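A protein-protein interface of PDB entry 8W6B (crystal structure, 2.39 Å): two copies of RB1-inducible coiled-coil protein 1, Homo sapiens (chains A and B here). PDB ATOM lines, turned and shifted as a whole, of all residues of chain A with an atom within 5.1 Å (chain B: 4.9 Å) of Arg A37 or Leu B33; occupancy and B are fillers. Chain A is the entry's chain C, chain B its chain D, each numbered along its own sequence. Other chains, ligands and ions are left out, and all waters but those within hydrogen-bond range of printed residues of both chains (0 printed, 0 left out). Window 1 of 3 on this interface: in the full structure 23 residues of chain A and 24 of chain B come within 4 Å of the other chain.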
ATOM      1  N   ILE A  30     -13.843 -31.212  25.593  1.00  0.00           N
ATOM      2  CA  ILE A  30     -15.256 -30.846  25.545  1.00  0.00           C
ATOM      3  C   ILE A  30     -15.638 -30.054  26.782  1.00  0.00           C
ATOM      4  O   ILE A  30     -16.372 -29.058  26.699  1.00  0.00           O
ATOM      5  CB  ILE A  30     -16.130 -32.102  25.391  1.00  0.00           C
ATOM      6  CG1 ILE A  30     -16.092 -32.572  23.937  1.00  0.00           C
ATOM      7  CG2 ILE A  30     -17.569 -31.801  25.827  1.00  0.00           C
ATOM      8  CD1 ILE A  30     -16.621 -33.961  23.742  1.00  0.00           C
ATOM      9  N   SER A  32     -13.689 -28.085  28.554  1.00  0.00           N
ATOM     10  CA  SER A  32     -13.170 -26.723  28.454  1.00  0.00           C
ATOM     11  C   SER A  32     -13.912 -25.908  27.394  1.00  0.00           C
ATOM     12  O   SER A  32     -14.331 -24.777  27.654  1.00  0.00           O
ATOM     13  CB  SER A  32     -11.671 -26.743  28.157  1.00  0.00           C
ATOM     14  OG  SER A  32     -11.072 -27.816  28.847  1.00  0.00           O
ATOM     15  N   LEU A  33     -14.057 -26.447  26.182  1.00  0.00           N
ATOM     16  CA  LEU A  33     -14.669 -25.672  25.104  1.00  0.00           C
ATOM     17  C   LEU A  33     -16.094 -25.272  25.450  1.00  0.00           C
ATOM     18  O   LEU A  33     -16.508 -24.134  25.189  1.00  0.00           O
ATOM     19  CB  LEU A  33     -14.659 -26.467  23.789  1.00  0.00           C
ATOM     20  CG  LEU A  33     -13.325 -26.767  23.090  1.00  0.00           C
ATOM     21  CD1 LEU A  33     -13.611 -27.812  22.050  1.00  0.00           C
ATOM     22  CD2 LEU A  33     -12.722 -25.538  22.455  1.00  0.00           C
ATOM     23  N   SER A  34     -16.861 -26.187  26.044  1.00  0.00           N
ATOM     24  CA  SER A  34     -18.269 -25.882  26.226  1.00  0.00           C
ATOM     25  C   SER A  34     -18.449 -24.805  27.289  1.00  0.00           C
ATOM     26  O   SER A  34     -19.218 -23.859  27.088  1.00  0.00           O
ATOM     27  CB  SER A  34     -19.061 -27.162  26.534  1.00  0.00           C
ATOM     28  OG  SER A  34     -18.638 -27.748  27.732  1.00  0.00           O
ATOM     29  N   GLU A  35     -17.689 -24.875  28.384  1.00  0.00           N
ATOM     30  CA  GLU A  35     -17.777 -23.821  29.394  1.00  0.00           C
ATOM     31  C   GLU A  35     -17.258 -22.489  28.857  1.00  0.00           C
ATOM     32  O   GLU A  35     -17.919 -21.452  29.004  1.00  0.00           O
ATOM     33  CB  GLU A  35     -17.028 -24.220  30.666  1.00  0.00           C
ATOM     34  CG  GLU A  35     -17.451 -23.466  31.967  1.00  0.00           C
ATOM     35  CD  GLU A  35     -18.940 -23.009  32.066  1.00  0.00           C
ATOM     36  OE1 GLU A  35     -19.867 -23.825  31.851  1.00  0.00           O
ATOM     37  OE2 GLU A  35     -19.182 -21.820  32.405  1.00  0.00           O
ATOM     38  N   ASP A  36     -16.090 -22.489  28.213  1.00  0.00           N
ATOM     39  CA  ASP A  36     -15.574 -21.206  27.739  1.00  0.00           C
ATOM     40  C   ASP A  36     -16.441 -20.644  26.613  1.00  0.00           C
ATOM     41  O   ASP A  36     -16.633 -19.425  26.532  1.00  0.00           O
ATOM     42  CB  ASP A  36     -14.114 -21.343  27.294  1.00  0.00           C
ATOM     43  CG  ASP A  36     -13.472 -19.992  26.938  1.00  0.00           C
ATOM     44  OD1 ASP A  36     -12.910 -19.875  25.826  1.00  0.00           O
ATOM     45  OD2 ASP A  36     -13.525 -19.051  27.763  1.00  0.00           O
ATOM     46  N   ARG A  37     -16.995 -21.507  25.754  1.00  0.00           N
ATOM     47  CA  ARG A  37     -17.887 -21.002  24.720  1.00  0.00           C
ATOM     48  C   ARG A  37     -19.106 -20.349  25.338  1.00  0.00           C
ATOM     49  O   ARG A  37     -19.533 -19.275  24.896  1.00  0.00           O
ATOM     50  CB  ARG A  37     -18.306 -22.114  23.769  1.00  0.00           C
ATOM     51  CG  ARG A  37     -19.268 -21.648  22.744  1.00  0.00           C
ATOM     52  CD  ARG A  37     -19.248 -22.574  21.539  1.00  0.00           C
ATOM     53  NE  ARG A  37     -20.389 -22.265  20.703  1.00  0.00           N
ATOM     54  CZ  ARG A  37     -21.643 -22.585  21.014  1.00  0.00           C
ATOM     55  NH1 ARG A  37     -21.910 -23.256  22.127  1.00  0.00           N
ATOM     56  NH2 ARG A  37     -22.616 -22.250  20.191  1.00  0.00           N
ATOM     57  N   ALA A  38     -19.671 -20.975  26.375  1.00  0.00           N
ATOM     58  CA  ALA A  38     -20.758 -20.344  27.123  1.00  0.00           C
ATOM     59  C   ALA A  38     -20.382 -18.936  27.568  1.00  0.00           C
ATOM     60  O   ALA A  38     -21.161 -17.994  27.385  1.00  0.00           O
ATOM     61  CB  ALA A  38     -21.139 -21.189  28.340  1.00  0.00           C
ATOM     62  N   ARG A  39     -19.182 -18.760  28.136  1.00  0.00           N
ATOM     63  CA  ARG A  39     -18.856 -17.428  28.641  1.00  0.00           C
ATOM     64  C   ARG A  39     -18.636 -16.445  27.503  1.00  0.00           C
ATOM     65  O   ARG A  39     -19.080 -15.297  27.581  1.00  0.00           O
ATOM     66  CB  ARG A  39     -17.661 -17.457  29.583  1.00  0.00           C
ATOM     67  CG  ARG A  39     -17.967 -18.203  30.870  1.00  0.00           C
ATOM     68  CD  ARG A  39     -16.747 -18.319  31.766  1.00  0.00           C
ATOM     69  NE  ARG A  39     -15.927 -19.450  31.348  1.00  0.00           N
ATOM     70  CZ  ARG A  39     -15.578 -20.469  32.128  1.00  0.00           C
ATOM     71  NH1 ARG A  39     -14.825 -21.445  31.627  1.00  0.00           N
ATOM     72  NH2 ARG A  39     -15.996 -20.525  33.389  1.00  0.00           N
ATOM     73  N   LEU A  40     -18.017 -16.886  26.409  1.00  0.00           N
ATOM     74  CA  LEU A  40     -17.906 -16.020  25.240  1.00  0.00           C
ATOM     75  C   LEU A  40     -19.281 -15.604  24.745  1.00  0.00           C
ATOM     76  O   LEU A  40     -19.473 -14.462  24.312  1.00  0.00           O
ATOM     77  CB  LEU A  40     -17.130 -16.717  24.120  1.00  0.00           C
ATOM     78  CG  LEU A  40     -15.650 -16.883  24.409  1.00  0.00           C
ATOM     79  CD1 LEU A  40     -15.021 -17.813  23.371  1.00  0.00           C
ATOM     80  CD2 LEU A  40     -14.955 -15.524  24.439  1.00  0.00           C
ATOM     81  N   LEU A  41     -20.262 -16.505  24.831  1.00  0.00           N
ATOM     82  CA  LEU A  41     -21.617 -16.134  24.443  1.00  0.00           C
ATOM     83  C   LEU A  41     -22.135 -14.986  25.297  1.00  0.00           C
ATOM     84  O   LEU A  41     -22.633 -13.982  24.766  1.00  0.00           O
ATOM     85  CB  LEU A  41     -22.543 -17.341  24.527  1.00  0.00           C
ATOM     86  CG  LEU A  41     -22.878 -17.969  23.173  1.00  0.00           C
ATOM     87  CD1 LEU A  41     -23.954 -19.027  23.343  1.00  0.00           C
ATOM     88  CD2 LEU A  41     -23.310 -16.915  22.172  1.00  0.00           C
ATOM     89  N   LEU B  29     -19.259 -32.799  18.190  1.00  0.00           N
ATOM     90  CA  LEU B  29     -19.348 -31.699  19.146  1.00  0.00           C
ATOM     91  C   LEU B  29     -18.076 -30.854  19.146  1.00  0.00           C
ATOM     92  O   LEU B  29     -18.142 -29.622  19.080  1.00  0.00           O
ATOM     93  CB  LEU B  29     -19.627 -32.242  20.542  1.00  0.00           C
ATOM     94  CG  LEU B  29     -19.841 -31.139  21.567  1.00  0.00           C
ATOM     95  CD1 LEU B  29     -21.057 -30.346  21.173  1.00  0.00           C
ATOM     96  CD2 LEU B  29     -20.002 -31.727  22.968  1.00  0.00           C
ATOM     97  N   ILE B  30     -16.914 -31.504  19.253  1.00  0.00           N
ATOM     98  CA  ILE B  30     -15.638 -30.795  19.275  1.00  0.00           C
ATOM     99  C   ILE B  30     -15.483 -29.937  18.022  1.00  0.00           C
ATOM    100  O   ILE B  30     -15.034 -28.786  18.090  1.00  0.00           O
ATOM    101  CB  ILE B  30     -14.470 -31.796  19.418  1.00  0.00           C
ATOM    102  CG1 ILE B  30     -14.357 -32.279  20.871  1.00  0.00           C
ATOM    103  CG2 ILE B  30     -13.176 -31.154  18.961  1.00  0.00           C
ATOM    104  CD1 ILE B  30     -13.564 -33.538  21.072  1.00  0.00           C
ATOM    105  N   GLU B  31     -15.884 -30.473  16.868  1.00  0.00           N
ATOM    106  CA  GLU B  31     -15.795 -29.717  15.623  1.00  0.00           C
ATOM    107  C   GLU B  31     -16.703 -28.496  15.643  1.00  0.00           C
ATOM    108  O   GLU B  31     -16.286 -27.402  15.258  1.00  0.00           O
ATOM    109  CB  GLU B  31     -16.107 -30.632  14.426  1.00  0.00           C
ATOM    110  CG  GLU B  31     -14.817 -31.198  13.818  1.00  0.00           C
ATOM    111  CD  GLU B  31     -15.020 -32.195  12.704  1.00  0.00           C
ATOM    112  OE1 GLU B  31     -16.147 -32.323  12.182  1.00  0.00           O
ATOM    113  OE2 GLU B  31     -14.022 -32.843  12.336  1.00  0.00           O
ATOM    114  N   SER B  32     -17.955 -28.652  16.085  1.00  0.00           N
ATOM    115  CA  SER B  32     -18.833 -27.483  16.169  1.00  0.00           C
ATOM    116  C   SER B  32     -18.336 -26.497  17.218  1.00  0.00           C
ATOM    117  O   SER B  32     -18.202 -25.302  16.937  1.00  0.00           O
ATOM    118  CB  SER B  32     -20.278 -27.883  16.478  1.00  0.00           C
ATOM    119  OG  SER B  32     -20.605 -29.046  15.779  1.00  0.00           O
ATOM    120  N   LEU B  33     -18.050 -26.979  18.435  1.00  0.00           N
ATOM    121  CA  LEU B  33     -17.587 -26.073  19.487  1.00  0.00           C
ATOM    122  C   LEU B  33     -16.302 -25.343  19.080  1.00  0.00           C
ATOM    123  O   LEU B  33     -16.196 -24.125  19.270  1.00  0.00           O
ATOM    124  CB  LEU B  33     -17.381 -26.831  20.794  1.00  0.00           C
ATOM    125  CG  LEU B  33     -18.602 -27.448  21.499  1.00  0.00           C
ATOM    126  CD1 LEU B  33     -18.121 -28.324  22.639  1.00  0.00           C
ATOM    127  CD2 LEU B  33     -19.602 -26.409  22.023  1.00  0.00           C
ATOM    128  N   SER B  34     -15.333 -26.065  18.497  1.00  0.00           N
ATOM    129  CA  SER B  34     -14.061 -25.451  18.092  1.00  0.00           C
ATOM    130  C   SER B  34     -14.284 -24.274  17.160  1.00  0.00           C
ATOM    131  O   SER B  34     -13.768 -23.174  17.394  1.00  0.00           O
ATOM    132  CB  SER B  34     -13.169 -26.464  17.365  1.00  0.00           C
ATOM    133  OG  SER B  34     -12.629 -27.398  18.253  1.00  0.00           O
ATOM    134  N   GLU B  35     -15.018 -24.510  16.066  1.00  0.00           N
ATOM    135  CA  GLU B  35     -15.174 -23.474  15.055  1.00  0.00           C
ATOM    136  C   GLU B  35     -16.001 -22.308  15.581  1.00  0.00           C
ATOM    137  O   GLU B  35     -15.710 -21.151  15.268  1.00  0.00           O
ATOM    138  CB  GLU B  35     -15.813 -24.053  13.795  1.00  0.00           C
ATOM    139  CG  GLU B  35     -14.912 -24.936  12.972  1.00  0.00           C
ATOM    140  CD  GLU B  35     -15.700 -25.940  12.122  1.00  0.00           C
ATOM    141  OE1 GLU B  35     -15.226 -27.092  11.943  1.00  0.00           O
ATOM    142  OE2 GLU B  35     -16.798 -25.576  11.635  1.00  0.00           O
ATOM    143  N   ASP B  36     -17.052 -22.586  16.354  1.00  0.00           N
ATOM    144  CA  ASP B  36     -17.922 -21.500  16.794  1.00  0.00           C
ATOM    145  C   ASP B  36     -17.219 -20.631  17.820  1.00  0.00           C
ATOM    146  O   ASP B  36     -17.349 -19.402  17.802  1.00  0.00           O
ATOM    147  CB  ASP B  36     -19.226 -22.046  17.375  1.00  0.00           C
ATOM    148  CG  ASP B  36     -20.265 -20.948  17.606  1.00  0.00           C
ATOM    149  OD1 ASP B  36     -20.908 -20.926  18.685  1.00  0.00           O
ATOM    150  OD2 ASP B  36     -20.435 -20.102  16.695  1.00  0.00           O
ATOM    151  N   ARG B  37     -16.482 -21.261  18.731  1.00  0.00           N
ATOM    152  CA  ARG B  37     -15.690 -20.514  19.694  1.00  0.00           C
ATOM    153  C   ARG B  37     -14.692 -19.614  18.981  1.00  0.00           C
ATOM    154  O   ARG B  37     -14.537 -18.437  19.329  1.00  0.00           O
ATOM    155  CB  ARG B  37     -14.985 -21.497  20.622  1.00  0.00           C
ATOM    156  CG  ARG B  37     -14.505 -20.893  21.853  1.00  0.00           C
ATOM    157  CD  ARG B  37     -14.145 -21.924  22.848  1.00  0.00           C
ATOM    158  NE  ARG B  37     -13.078 -21.370  23.642  1.00  0.00           N
ATOM    159  CZ  ARG B  37     -11.798 -21.427  23.301  1.00  0.00           C
ATOM    160  NH1 ARG B  37     -10.881 -20.891  24.093  1.00  0.00           N
ATOM    161  NH2 ARG B  37     -11.436 -22.061  22.199  1.00  0.00           N
ATOM    162  N   ALA B  38     -14.029 -20.143  17.953  1.00  0.00           N
ATOM    163  CA  ALA B  38     -13.118 -19.327  17.164  1.00  0.00           C
ATOM    164  C   ALA B  38     -13.831 -18.097  16.624  1.00  0.00           C
ATOM    165  O   ALA B  38     -13.338 -16.971  16.770  1.00  0.00           O
ATOM    166  CB  ALA B  38     -12.513 -20.158  16.031  1.00  0.00           C
ATOM    167  N   LEU B  40     -16.516 -16.695  17.775  1.00  0.00           N
ATOM    168  CA  LEU B  40     -16.953 -15.819  18.855  1.00  0.00           C
ATOM    169  C   LEU B  40     -15.805 -14.946  19.327  1.00  0.00           C
ATOM    170  O   LEU B  40     -15.993 -13.750  19.584  1.00  0.00           O
ATOM    171  CB  LEU B  40     -17.518 -16.629  20.026  1.00  0.00           C
ATOM    172  CG  LEU B  40     -18.930 -17.216  19.948  1.00  0.00           C
ATOM    173  CD1 LEU B  40     -19.271 -17.951  21.242  1.00  0.00           C
ATOM    174  CD2 LEU B  40     -19.944 -16.136  19.681  1.00  0.00           C
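The guanidinium group of Arg B37 lies within salt-bridge range of the side-chain carboxylate of Asp A36, at 2.7 Å.
The guanidinium group (NE) of Arg A37 lies within salt-bridge range of the side-chain carboxylate (OD1) of Asp B36, 2.5 Å away.
OG of Ser A34 is in hydrogen-bond range of O of Ile A30 (2.8 Å).
The backbone carbonyl oxygen of Ile B30 sits at hydrogen-bond distance from the side-chain hydroxyl of Ser B34 (2.8 Å).
Among the printed residues, pairs that only touch across the chains: Ile A30 with Leu B29 (3.8 Å), Ile A30 with Ile B30 (3.5 Å), Leu A33 with Ser B34 (3.9 Å), Leu A33 with Arg B37 (3.7 Å), Arg A37 with Leu B33 (3.9 Å), Arg A37 with Leu B40 (3.9 Å), Leu A40 with Arg B37 (3.5 Å), Leu A40 with Leu B40 (3.8 Å) and Leu A41 with Leu B40 (3.99 Å).
Of the printed residues of chain B, Leu A33 touches Ser B34 and Arg B37.
Arg A37 touches just these residues of chain B: Leu B33, Asp B36 and Leu B40.
Glu B31 touches none of the printed residues of chain A.
Leu B33 touches just one residue of chain A: Arg A37 (3.9 Å).
Of the printed residues of chain A, Leu B40 touches Arg A37 (3.9 Å), Leu A40 (3.8 Å) and Leu A41 (3.99 Å).
The nearest residue of chain A that does not touch Leu B33 is Leu A33 (4.1 Å).
Of the 11 printed residues of chain B, 7 touch a printed residue of chain A.
Hydrophobic or aromatic side chains of chain B that line the printed part of chain A: Leu B29, Ile B30, Leu B33 and Leu B40.
Of the 11 printed residues of chain A, 6 touch a printed residue of chain B.
Hydrophobic or aromatic side chains of chain A that line the printed part of chain B: Ile A30, Leu A33 and Leu A40.
Among the printed residues, 11 pairs touch across the chains.
Leu A33 touches Ser B34, but with the chains exchanged Ser A34 does not touch Leu B33 (4.2 Å).
Asp A36 touches Arg B37, and with the chains exchanged Arg A37 touches Asp B36.
Arg A37 touches Leu B40, and with the chains exchanged Leu A40 touches Arg B37.
Leu B40 touches its own counterpart, Leu A40.
Positions printed for both chains: 30, 32, 33, 34, 35, 36, 37, 38 and 40.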
